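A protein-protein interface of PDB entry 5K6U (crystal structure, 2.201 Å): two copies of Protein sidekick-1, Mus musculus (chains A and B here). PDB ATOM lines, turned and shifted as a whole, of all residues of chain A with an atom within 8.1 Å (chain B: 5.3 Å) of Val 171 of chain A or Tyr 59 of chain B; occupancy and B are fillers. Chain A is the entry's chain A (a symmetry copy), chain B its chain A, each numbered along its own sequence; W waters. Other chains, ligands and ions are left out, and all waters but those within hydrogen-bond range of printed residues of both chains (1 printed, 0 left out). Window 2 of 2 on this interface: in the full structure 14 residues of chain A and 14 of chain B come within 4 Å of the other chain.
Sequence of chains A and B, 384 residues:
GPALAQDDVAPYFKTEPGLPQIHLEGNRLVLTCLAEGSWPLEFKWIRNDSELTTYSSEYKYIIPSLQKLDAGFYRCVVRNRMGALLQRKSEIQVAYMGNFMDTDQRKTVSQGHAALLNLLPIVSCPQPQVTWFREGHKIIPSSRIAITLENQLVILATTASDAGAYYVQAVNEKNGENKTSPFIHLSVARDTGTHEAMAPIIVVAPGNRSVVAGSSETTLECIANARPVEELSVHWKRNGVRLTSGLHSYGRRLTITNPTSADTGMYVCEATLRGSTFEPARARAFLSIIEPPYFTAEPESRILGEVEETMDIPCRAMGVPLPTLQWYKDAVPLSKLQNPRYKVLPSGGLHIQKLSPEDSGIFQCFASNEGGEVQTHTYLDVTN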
ATOM      1  N   MET A  97      27.362   9.724  29.932  1.00  0.00           N
ATOM      2  CA  MET A  97      25.952   9.959  30.165  1.00  0.00           C
ATOM      3  C   MET A  97      25.757  10.288  31.631  1.00  0.00           C
ATOM      4  O   MET A  97      26.073   9.469  32.493  1.00  0.00           O
ATOM      5  CB  MET A  97      25.117   8.748  29.771  1.00  0.00           C
ATOM      6  CG  MET A  97      23.671   9.088  29.720  1.00  0.00           C
ATOM      7  SD  MET A  97      22.694   7.829  28.928  1.00  0.00           S
ATOM      8  CE  MET A  97      21.296   8.821  28.480  1.00  0.00           C
ATOM      9  N   PHE A 100      19.438  11.842  35.311  1.00  0.00           N
ATOM     10  CA  PHE A 100      18.322  12.764  35.417  1.00  0.00           C
ATOM     11  C   PHE A 100      18.254  13.313  36.835  1.00  0.00           C
ATOM     12  O   PHE A 100      18.691  12.667  37.792  1.00  0.00           O
ATOM     13  CB  PHE A 100      17.003  12.077  35.065  1.00  0.00           C
ATOM     14  CG  PHE A 100      16.894  11.670  33.627  1.00  0.00           C
ATOM     15  CD1 PHE A 100      16.534  12.592  32.667  1.00  0.00           C
ATOM     16  CD2 PHE A 100      17.141  10.358  33.246  1.00  0.00           C
ATOM     17  CE1 PHE A 100      16.424  12.219  31.348  1.00  0.00           C
ATOM     18  CE2 PHE A 100      17.039   9.978  31.933  1.00  0.00           C
ATOM     19  CZ  PHE A 100      16.681  10.907  30.977  1.00  0.00           C
ATOM     20  N   LEU A 119      12.245  16.684  27.296  1.00  0.00           N
ATOM     21  CA  LEU A 119      13.151  15.681  27.842  1.00  0.00           C
ATOM     22  C   LEU A 119      13.828  16.242  29.084  1.00  0.00           C
ATOM     23  O   LEU A 119      14.356  17.360  29.078  1.00  0.00           O
ATOM     24  CB  LEU A 119      14.202  15.267  26.806  1.00  0.00           C
ATOM     25  CG  LEU A 119      15.377  14.418  27.314  1.00  0.00           C
ATOM     26  CD1 LEU A 119      14.923  13.020  27.652  1.00  0.00           C
ATOM     27  CD2 LEU A 119      16.524  14.360  26.312  1.00  0.00           C
ATOM     28  N   ILE A 122      19.486  16.239  31.258  1.00  0.00           N
ATOM     29  CA  ILE A 122      20.480  15.180  31.388  1.00  0.00           C
ATOM     30  C   ILE A 122      21.670  15.517  30.501  1.00  0.00           C
ATOM     31  O   ILE A 122      21.510  15.794  29.307  1.00  0.00           O
ATOM     32  CB  ILE A 122      19.878  13.805  31.043  1.00  0.00           C
ATOM     33  CG1 ILE A 122      20.934  12.704  31.160  1.00  0.00           C
ATOM     34  CG2 ILE A 122      19.240  13.811  29.673  1.00  0.00           C
ATOM     35  CD1 ILE A 122      20.356  11.322  31.011  1.00  0.00           C
ATOM     36  N   SER A 124      24.770  14.479  28.354  1.00  0.00           N
ATOM     37  CA  SER A 124      25.165  13.277  27.620  1.00  0.00           C
ATOM     38  C   SER A 124      25.950  13.636  26.360  1.00  0.00           C
ATOM     39  O   SER A 124      25.559  14.544  25.622  1.00  0.00           O
ATOM     40  CB  SER A 124      23.943  12.447  27.230  1.00  0.00           C
ATOM     41  OG  SER A 124      24.304  11.326  26.427  1.00  0.00           O
ATOM     42  N   PRO A 126      27.411  11.400  23.015  1.00  0.00           N
ATOM     43  CA  PRO A 126      26.589  12.383  22.306  1.00  0.00           C
ATOM     44  C   PRO A 126      25.159  12.344  22.834  1.00  0.00           C
ATOM     45  O   PRO A 126      24.900  11.620  23.800  1.00  0.00           O
ATOM     46  CB  PRO A 126      26.663  11.914  20.861  1.00  0.00           C
ATOM     47  CG  PRO A 126      26.786  10.429  20.983  1.00  0.00           C
ATOM     48  CD  PRO A 126      27.591  10.168  22.226  1.00  0.00           C
ATOM     49  N   GLN A 127      24.258  13.110  22.235  1.00  0.00           N
ATOM     50  CA  GLN A 127      22.907  13.165  22.754  1.00  0.00           C
ATOM     51  C   GLN A 127      22.266  11.780  22.665  1.00  0.00           C
ATOM     52  O   GLN A 127      22.466  11.058  21.680  1.00  0.00           O
ATOM     53  CB  GLN A 127      22.083  14.198  21.989  1.00  0.00           C
ATOM     54  CG  GLN A 127      22.338  15.641  22.452  1.00  0.00           C
ATOM     55  CD  GLN A 127      22.013  15.860  23.927  1.00  0.00           C
ATOM     56  OE1 GLN A 127      20.845  15.872  24.324  1.00  0.00           O
ATOM     57  NE2 GLN A 127      23.051  16.033  24.744  1.00  0.00           N
ATOM     58  N   PRO A 128      21.502  11.374  23.667  1.00  0.00           N
ATOM     59  CA  PRO A 128      20.990  10.000  23.687  1.00  0.00           C
ATOM     60  C   PRO A 128      19.880   9.793  22.672  1.00  0.00           C
ATOM     61  O   PRO A 128      19.314  10.738  22.126  1.00  0.00           O
ATOM     62  CB  PRO A 128      20.458   9.841  25.112  1.00  0.00           C
ATOM     63  CG  PRO A 128      20.066  11.230  25.510  1.00  0.00           C
ATOM     64  CD  PRO A 128      21.075  12.147  24.844  1.00  0.00           C
ATOM     65  N   GLN A 129      19.603   8.522  22.410  1.00  0.00           N
ATOM     66  CA  GLN A 129      18.367   8.107  21.763  1.00  0.00           C
ATOM     67  C   GLN A 129      17.322   7.921  22.852  1.00  0.00           C
ATOM     68  O   GLN A 129      17.587   7.299  23.882  1.00  0.00           O
ATOM     69  CB  GLN A 129      18.549   6.810  20.977  1.00  0.00           C
ATOM     70  N   VAL A 130      16.142   8.461  22.623  1.00  0.00           N
ATOM     71  CA  VAL A 130      15.110   8.581  23.637  1.00  0.00           C
ATOM     72  C   VAL A 130      13.882   7.812  23.181  1.00  0.00           C
ATOM     73  O   VAL A 130      13.412   8.004  22.055  1.00  0.00           O
ATOM     74  CB  VAL A 130      14.776  10.059  23.875  1.00  0.00           C
ATOM     75  CG1 VAL A 130      13.462  10.202  24.537  1.00  0.00           C
ATOM     76  CG2 VAL A 130      15.892  10.722  24.675  1.00  0.00           C
ATOM     77  N   THR A 131      13.354   6.962  24.056  1.00  0.00           N
ATOM     78  CA  THR A 131      12.054   6.341  23.869  1.00  0.00           C
ATOM     79  C   THR A 131      11.133   6.840  24.968  1.00  0.00           C
ATOM     80  O   THR A 131      11.488   6.757  26.145  1.00  0.00           O
ATOM     81  CB  THR A 131      12.140   4.812  23.916  1.00  0.00           C
ATOM     82  OG1 THR A 131      13.139   4.356  22.994  1.00  0.00           O
ATOM     83  CG2 THR A 131      10.815   4.220  23.526  1.00  0.00           C
ATOM     84  N   ASN A 151      14.238  15.369  20.932  1.00  0.00           N
ATOM     85  CA  ASN A 151      13.698  14.340  21.810  1.00  0.00           C
ATOM     86  C   ASN A 151      12.528  14.813  22.654  1.00  0.00           C
ATOM     87  O   ASN A 151      12.213  14.193  23.672  1.00  0.00           O
ATOM     88  CB  ASN A 151      14.790  13.784  22.723  1.00  0.00           C
ATOM     89  CG  ASN A 151      15.828  13.024  21.959  1.00  0.00           C
ATOM     90  OD1 ASN A 151      15.507  12.348  20.985  1.00  0.00           O
ATOM     91  ND2 ASN A 151      17.077  13.129  22.386  1.00  0.00           N
ATOM     92  N   VAL A 168      10.831   8.638  30.146  1.00  0.00           N
ATOM     93  CA  VAL A 168      11.760   8.345  29.066  1.00  0.00           C
ATOM     94  C   VAL A 168      12.735   7.240  29.467  1.00  0.00           C
ATOM     95  O   VAL A 168      13.129   7.135  30.634  1.00  0.00           O
ATOM     96  CB  VAL A 168      12.511   9.641  28.696  1.00  0.00           C
ATOM     97  CG1 VAL A 168      13.958   9.385  28.404  1.00  0.00           C
ATOM     98  CG2 VAL A 168      11.809  10.331  27.559  1.00  0.00           C
ATOM     99  N   GLN A 169      13.123   6.416  28.499  1.00  0.00           N
ATOM    100  CA  GLN A 169      14.377   5.672  28.551  1.00  0.00           C
ATOM    101  C   GLN A 169      15.360   6.338  27.591  1.00  0.00           C
ATOM    102  O   GLN A 169      15.111   6.401  26.380  1.00  0.00           O
ATOM    103  CB  GLN A 169      14.184   4.201  28.179  1.00  0.00           C
ATOM    104  CG  GLN A 169      13.413   3.387  29.194  1.00  0.00           C
ATOM    105  CD  GLN A 169      13.216   1.931  28.767  1.00  0.00           C
ATOM    106  OE1 GLN A 169      13.730   1.501  27.732  1.00  0.00           O
ATOM    107  NE2 GLN A 169      12.462   1.173  29.564  1.00  0.00           N
ATOM    108  N   ALA A 170      16.466   6.841  28.125  1.00  0.00           N
ATOM    109  CA  ALA A 170      17.489   7.483  27.315  1.00  0.00           C
ATOM    110  C   ALA A 170      18.670   6.534  27.154  1.00  0.00           C
ATOM    111  O   ALA A 170      19.152   5.951  28.136  1.00  0.00           O
ATOM    112  CB  ALA A 170      17.930   8.797  27.948  1.00  0.00           C
ATOM    113  N   VAL A 171      19.118   6.353  25.919  1.00  0.00           N
ATOM    114  CA  VAL A 171      20.216   5.437  25.633  1.00  0.00           C
ATOM    115  C   VAL A 171      21.357   6.207  24.980  1.00  0.00           C
ATOM    116  O   VAL A 171      21.168   6.839  23.935  1.00  0.00           O
ATOM    117  CB  VAL A 171      19.758   4.275  24.749  1.00  0.00           C
ATOM    118  CG1 VAL A 171      20.966   3.450  24.329  1.00  0.00           C
ATOM    119  CG2 VAL A 171      18.760   3.437  25.508  1.00  0.00           C
ATOM    120  N   ASN A 172      22.542   6.151  25.586  1.00  0.00           N
ATOM    121  CA  ASN A 172      23.747   6.618  24.903  1.00  0.00           C
ATOM    122  C   ASN A 172      24.233   5.525  23.958  1.00  0.00           C
ATOM    123  O   ASN A 172      24.706   4.470  24.399  1.00  0.00           O
ATOM    124  CB  ASN A 172      24.835   7.007  25.892  1.00  0.00           C
ATOM    125  CG  ASN A 172      26.059   7.605  25.204  1.00  0.00           C
ATOM    126  OD1 ASN A 172      26.673   6.982  24.327  1.00  0.00           O
ATOM    127  ND2 ASN A 172      26.416   8.826  25.597  1.00  0.00           N
ATOM    128  N   GLU A 173      24.144   5.779  22.652  1.00  0.00           N
ATOM    129  CA  GLU A 173      24.457   4.745  21.675  1.00  0.00           C
ATOM    130  C   GLU A 173      25.952   4.462  21.544  1.00  0.00           C
ATOM    131  O   GLU A 173      26.315   3.437  20.967  1.00  0.00           O
ATOM    132  CB  GLU A 173      23.896   5.142  20.306  1.00  0.00           C
ATOM    133  CG  GLU A 173      24.797   6.122  19.559  1.00  0.00           C
ATOM    134  CD  GLU A 173      24.077   6.863  18.450  1.00  0.00           C
ATOM    135  OE1 GLU A 173      22.835   6.734  18.352  1.00  0.00           O
ATOM    136  OE2 GLU A 173      24.758   7.577  17.682  1.00  0.00           O
ATOM    137  N   LYS A 174      26.829   5.337  22.050  1.00  0.00           N
ATOM    138  CA  LYS A 174      28.262   5.095  21.897  1.00  0.00           C
ATOM    139  C   LYS A 174      28.845   4.234  23.007  1.00  0.00           C
ATOM    140  O   LYS A 174      29.686   3.373  22.734  1.00  0.00           O
ATOM    141  CB  LYS A 174      29.033   6.412  21.837  1.00  0.00           C
ATOM    142  CG  LYS A 174      28.783   7.199  20.570  1.00  0.00           C
ATOM    143  CD  LYS A 174      29.285   6.458  19.340  1.00  0.00           C
ATOM    144  CE  LYS A 174      28.889   7.206  18.079  1.00  0.00           C
ATOM    145  NZ  LYS A 174      29.571   6.640  16.894  1.00  0.00           N
ATOM    146  N   ASN A 175      28.451   4.452  24.261  1.00  0.00           N
ATOM    147  CA  ASN A 175      28.932   3.616  25.357  1.00  0.00           C
ATOM    148  C   ASN A 175      27.892   2.615  25.843  1.00  0.00           C
ATOM    149  O   ASN A 175      28.171   1.853  26.769  1.00  0.00           O
ATOM    150  CB  ASN A 175      29.424   4.481  26.536  1.00  0.00           C
ATOM    151  CG  ASN A 175      28.314   5.321  27.183  1.00  0.00           C
ATOM    152  OD1 ASN A 175      27.125   5.128  26.933  1.00  0.00           O
ATOM    153  ND2 ASN A 175      28.713   6.259  28.028  1.00  0.00           N
ATOM    154  N   GLY A 176      26.695   2.613  25.263  1.00  0.00           N
ATOM    155  CA  GLY A 176      25.693   1.634  25.601  1.00  0.00           C
ATOM    156  C   GLY A 176      24.878   1.907  26.852  1.00  0.00           C
ATOM    157  O   GLY A 176      23.868   1.227  27.062  1.00  0.00           O
ATOM    158  N   GLU A 177      25.268   2.868  27.687  1.00  0.00           N
ATOM    159  CA  GLU A 177      24.548   3.119  28.932  1.00  0.00           C
ATOM    160  C   GLU A 177      23.135   3.648  28.675  1.00  0.00           C
ATOM    161  O   GLU A 177      22.867   4.340  27.683  1.00  0.00           O
ATOM    162  CB  GLU A 177      25.318   4.114  29.798  1.00  0.00           C
ATOM    163  CG  GLU A 177      26.668   3.581  30.253  1.00  0.00           C
ATOM    164  CD  GLU A 177      27.570   4.650  30.868  1.00  0.00           C
ATOM    165  OE1 GLU A 177      27.082   5.771  31.140  1.00  0.00           O
ATOM    166  OE2 GLU A 177      28.771   4.363  31.072  1.00  0.00           O
ATOM    167  N   ASN A 178      22.225   3.318  29.595  1.00  0.00           N
ATOM    168  CA  ASN A 178      20.837   3.750  29.524  1.00  0.00           C
ATOM    169  C   ASN A 178      20.371   4.254  30.883  1.00  0.00           C
ATOM    170  O   ASN A 178      20.804   3.769  31.928  1.00  0.00           O
ATOM    171  CB  ASN A 178      19.905   2.619  29.043  1.00  0.00           C
ATOM    172  CG  ASN A 178      19.893   1.438  29.975  1.00  0.00           C
ATOM    173  OD1 ASN A 178      19.341   1.507  31.068  1.00  0.00           O
ATOM    174  ND2 ASN A 178      20.489   0.330  29.544  1.00  0.00           N
ATOM    175  N   LYS A 179      19.485   5.240  30.859  1.00  0.00           N
ATOM    176  CA  LYS A 179      18.896   5.788  32.073  1.00  0.00           C
ATOM    177  C   LYS A 179      17.400   5.952  31.856  1.00  0.00           C
ATOM    178  O   LYS A 179      16.960   6.300  30.754  1.00  0.00           O
ATOM    179  CB  LYS A 179      19.490   7.155  32.458  1.00  0.00           C
ATOM    180  CG  LYS A 179      21.006   7.231  32.554  1.00  0.00           C
ATOM    181  CD  LYS A 179      21.502   6.689  33.872  1.00  0.00           C
ATOM    182  CE  LYS A 179      22.937   7.091  34.121  1.00  0.00           C
ATOM    183  NZ  LYS A 179      23.419   6.442  35.360  1.00  0.00           N
ATOM    184  N   THR A 180      16.635   5.712  32.917  1.00  0.00           N
ATOM    185  CA  THR A 180      15.215   6.003  32.972  1.00  0.00           C
ATOM    186  C   THR A 180      15.009   7.288  33.757  1.00  0.00           C
ATOM    187  O   THR A 180      15.606   7.476  34.818  1.00  0.00           O
ATOM    188  CB  THR A 180      14.447   4.863  33.639  1.00  0.00           C
ATOM    189  OG1 THR A 180      14.558   3.679  32.845  1.00  0.00           O
ATOM    190  CG2 THR A 180      12.979   5.232  33.809  1.00  0.00           C
ATOM    191  N   LEU B  31      29.721  -2.447  20.203  1.00  0.00           N
ATOM    192  CA  LEU B  31      28.998  -2.449  18.935  1.00  0.00           C
ATOM    193  C   LEU B  31      27.490  -2.382  19.198  1.00  0.00           C
ATOM    194  O   LEU B  31      27.004  -2.858  20.227  1.00  0.00           O
ATOM    195  CB  LEU B  31      29.321  -3.687  18.105  1.00  0.00           C
ATOM    196  CG  LEU B  31      30.823  -3.912  17.959  1.00  0.00           C
ATOM    197  CD1 LEU B  31      31.114  -5.228  17.274  1.00  0.00           C
ATOM    198  CD2 LEU B  31      31.439  -2.770  17.194  1.00  0.00           C
ATOM    199  N   THR B  32      26.758  -1.769  18.274  1.00  0.00           N
ATOM    200  CA  THR B  32      25.352  -1.495  18.465  1.00  0.00           C
ATOM    201  C   THR B  32      24.596  -1.757  17.163  1.00  0.00           C
ATOM    202  O   THR B  32      25.104  -1.441  16.088  1.00  0.00           O
ATOM    203  CB  THR B  32      25.135  -0.034  18.837  1.00  0.00           C
ATOM    204  OG1 THR B  32      25.624   0.814  17.779  1.00  0.00           O
ATOM    205  CG2 THR B  32      25.826   0.310  20.142  1.00  0.00           C
ATOM    206  N   CYS B  33      23.366  -2.275  17.244  1.00  0.00           N
ATOM    207  CA  CYS B  33      22.542  -2.529  16.075  1.00  0.00           C
ATOM    208  C   CYS B  33      21.352  -1.592  16.175  1.00  0.00           C
ATOM    209  O   CYS B  33      20.370  -1.897  16.855  1.00  0.00           O
ATOM    210  CB  CYS B  33      22.139  -3.927  16.087  1.00  0.00           C
ATOM    211  SG  CYS B  33      21.597  -4.572  14.588  1.00  0.00           S
ATOM    212  N   LEU B  34      21.506  -0.398  15.600  1.00  0.00           N
ATOM    213  CA  LEU B  34      20.582   0.708  15.772  1.00  0.00           C
ATOM    214  C   LEU B  34      19.476   0.674  14.715  1.00  0.00           C
ATOM    215  O   LEU B  34      19.388   1.512  13.813  1.00  0.00           O
ATOM    216  CB  LEU B  34      21.340   2.028  15.741  1.00  0.00           C
ATOM    217  CG  LEU B  34      22.427   2.112  16.813  1.00  0.00           C
ATOM    218  CD1 LEU B  34      23.368   3.301  16.597  1.00  0.00           C
ATOM    219  CD2 LEU B  34      21.804   2.181  18.207  1.00  0.00           C
ATOM    220  N   PHE B  43      17.879  -9.190  17.098  1.00  0.00           N
ATOM    221  CA  PHE B  43      19.204  -8.868  16.596  1.00  0.00           C
ATOM    222  C   PHE B  43      20.144 -10.039  16.842  1.00  0.00           C
ATOM    223  O   PHE B  43      20.093 -10.680  17.892  1.00  0.00           O
ATOM    224  CB  PHE B  43      19.776  -7.629  17.291  1.00  0.00           C
ATOM    225  CG  PHE B  43      18.823  -6.474  17.367  1.00  0.00           C
ATOM    226  CD1 PHE B  43      17.936  -6.361  18.418  1.00  0.00           C
ATOM    227  CD2 PHE B  43      18.855  -5.478  16.409  1.00  0.00           C
ATOM    228  CE1 PHE B  43      17.064  -5.287  18.502  1.00  0.00           C
ATOM    229  CE2 PHE B  43      18.003  -4.410  16.479  1.00  0.00           C
ATOM    230  CZ  PHE B  43      17.094  -4.313  17.532  1.00  0.00           C
ATOM    231  N   TRP B  45      24.485 -11.192  16.013  1.00  0.00           N
ATOM    232  CA  TRP B  45      25.761 -10.676  15.547  1.00  0.00           C
ATOM    233  C   TRP B  45      26.519 -11.754  14.793  1.00  0.00           C
ATOM    234  O   TRP B  45      26.302 -12.954  14.992  1.00  0.00           O
ATOM    235  CB  TRP B  45      26.593 -10.130  16.706  1.00  0.00           C
ATOM    236  CG  TRP B  45      26.029  -8.823  17.178  1.00  0.00           C
ATOM    237  CD1 TRP B  45      25.081  -8.641  18.148  1.00  0.00           C
ATOM    238  CD2 TRP B  45      26.343  -7.520  16.668  1.00  0.00           C
ATOM    239  NE1 TRP B  45      24.793  -7.300  18.276  1.00  0.00           N
ATOM    240  CE2 TRP B  45      25.555  -6.591  17.381  1.00  0.00           C
ATOM    241  CE3 TRP B  45      27.214  -7.050  15.678  1.00  0.00           C
ATOM    242  CZ2 TRP B  45      25.620  -5.217  17.141  1.00  0.00           C
ATOM    243  CZ3 TRP B  45      27.280  -5.678  15.440  1.00  0.00           C
ATOM    244  CH2 TRP B  45      26.480  -4.781  16.163  1.00  0.00           C
ATOM    245  N   SER B  57      16.560  -9.718  21.867  1.00  0.00           N
ATOM    246  CA  SER B  57      16.204  -8.312  21.887  1.00  0.00           C
ATOM    247  C   SER B  57      17.382  -7.417  22.241  1.00  0.00           C
ATOM    248  O   SER B  57      17.211  -6.196  22.284  1.00  0.00           O
ATOM    249  CB  SER B  57      15.056  -8.074  22.882  1.00  0.00           C
ATOM    250  OG  SER B  57      15.478  -8.293  24.224  1.00  0.00           O
ATOM    251  N   GLU B  58      18.566  -7.978  22.473  1.00  0.00           N
ATOM    252  CA  GLU B  58      19.742  -7.179  22.798  1.00  0.00           C
ATOM    253  C   GLU B  58      20.432  -6.740  21.504  1.00  0.00           C
ATOM    254  O   GLU B  58      20.910  -7.575  20.728  1.00  0.00           O
ATOM    255  CB  GLU B  58      20.696  -7.962  23.702  1.00  0.00           C
ATOM    256  CG  GLU B  58      21.963  -7.206  24.064  1.00  0.00           C
ATOM    257  CD  GLU B  58      21.693  -5.833  24.669  1.00  0.00           C
ATOM    258  OE1 GLU B  58      21.295  -5.758  25.851  1.00  0.00           O
ATOM    259  OE2 GLU B  58      21.878  -4.823  23.956  1.00  0.00           O
ATOM    260  N   TYR B  59      20.476  -5.431  21.264  1.00  0.00           N
ATOM    261  CA  TYR B  59      21.095  -4.910  20.050  1.00  0.00           C
ATOM    262  C   TYR B  59      22.568  -4.558  20.229  1.00  0.00           C
ATOM    263  O   TYR B  59      23.220  -4.172  19.248  1.00  0.00           O
ATOM    264  CB  TYR B  59      20.349  -3.670  19.564  1.00  0.00           C
ATOM    265  CG  TYR B  59      20.257  -2.610  20.625  1.00  0.00           C
ATOM    266  CD1 TYR B  59      19.166  -2.559  21.477  1.00  0.00           C
ATOM    267  CD2 TYR B  59      21.269  -1.665  20.785  1.00  0.00           C
ATOM    268  CE1 TYR B  59      19.075  -1.599  22.455  1.00  0.00           C
ATOM    269  CE2 TYR B  59      21.186  -0.702  21.770  1.00  0.00           C
ATOM    270  CZ  TYR B  59      20.087  -0.680  22.600  1.00  0.00           C
ATOM    271  OH  TYR B  59      19.976   0.275  23.582  1.00  0.00           O
ATOM    272  N   LYS B  60      23.097  -4.657  21.444  1.00  0.00           N
ATOM    273  CA  LYS B  60      24.494  -4.380  21.717  1.00  0.00           C
ATOM    274  C   LYS B  60      25.323  -5.657  21.740  1.00  0.00           C
ATOM    275  O   LYS B  60      24.864  -6.722  22.168  1.00  0.00           O
ATOM    276  CB  LYS B  60      24.667  -3.664  23.059  1.00  0.00           C
ATOM    277  CG  LYS B  60      24.017  -2.306  23.134  1.00  0.00           C
ATOM    278  CD  LYS B  60      24.461  -1.608  24.395  1.00  0.00           C
ATOM    279  CE  LYS B  60      24.167  -2.461  25.607  1.00  0.00           C
ATOM    280  NZ  LYS B  60      22.706  -2.604  25.764  1.00  0.00           N
ATOM    281  N   TYR B  61      26.561  -5.535  21.280  1.00  0.00           N
ATOM    282  CA  TYR B  61      27.573  -6.566  21.472  1.00  0.00           C
ATOM    283  C   TYR B  61      28.804  -5.872  22.033  1.00  0.00           C
ATOM    284  O   TYR B  61      29.339  -4.947  21.408  1.00  0.00           O
ATOM    285  CB  TYR B  61      27.901  -7.300  20.167  1.00  0.00           C
ATOM    286  CG  TYR B  61      28.830  -8.466  20.370  1.00  0.00           C
ATOM    287  CD1 TYR B  61      28.326  -9.725  20.665  1.00  0.00           C
ATOM    288  CD2 TYR B  61      30.212  -8.307  20.307  1.00  0.00           C
ATOM    289  CE1 TYR B  61      29.168 -10.809  20.868  1.00  0.00           C
ATOM    290  CE2 TYR B  61      31.073  -9.391  20.508  1.00  0.00           C
ATOM    291  CZ  TYR B  61      30.537 -10.640  20.793  1.00  0.00           C
ATOM    292  OH  TYR B  61      31.350 -11.738  20.992  1.00  0.00           O
HETATM  293  O   HOH W   1      21.739  -0.211  25.532  1.00  0.00           O
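Water W1 lies within hydrogen-bond range of NZ of Lys 60 of chain B (2.6 Å), OH of Tyr 59 of chain B (2.7 Å) and O of Gly 176 of chain A (3.0 Å).
Val 171 of chain A touches just one residue of chain B: Tyr 59. Of chain A, only Val 171 (3.4 Å) comes within 4 Å of Tyr 59 of chain B. Printed residues of chain B within 4 Å of Gly 176 of chain A: Lys 60. Printed residues of chain A within 4 Å of Lys 60 of chain B: Gly 176. Printed residues of chain B within 4 Å of Glu 173 of chain A: Thr 32 and Leu 34. Of the printed residues of chain A, Leu 34 of chain B touches Glu 173. Trp 45 of chain B touches none of the printed residues of chain A. The nearest printed residue of chain B that does not touch Glu 173 of chain A is Leu 31 of chain B (6.2 Å).
No position is printed for both chains. Of the 4 pairs that touch across the chains among the printed residues, none has its exchanged pair printed and touching as well.
The backbone NH (N) of Cys 33 of chain B sits at hydrogen-bond distance from the backbone carbonyl oxygen (O) of Tyr 59 of chain B. The side-chain amino group (NZ) of Lys 60 of chain B is in salt-bridge range of the side-chain carboxylate (OE2) of Glu 58 of chain B, 3.0 Å away. The backbone carbonyl oxygen (O) of Gln 129 of chain A lies within hydrogen-bond range of the backbone NH (N) of Val 171 of chain A (2.7 Å).
Val 171 of chain A touches Tyr 59 of chain B. CG2 of Thr 32 of chain B touches O of Glu 173 of chain A, 3.3 Å away. OE1 of Glu 173 of chain A touches CD1 of Leu 34 of chain B (3.9 Å). Gly 176 of chain A touches Lys 60 of chain B.
Of the 11 printed residues of chain B, 4 touch a printed residue of chain A. Printed residues of chain A that touch a printed residue of chain B: Val 171, Glu 173 and Gly 176. Hydrophobic or aromatic side chains of chain A within 4 Å of the printed part of chain B: Val 171. Among the printed residues, 4 pairs touch across the chains.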
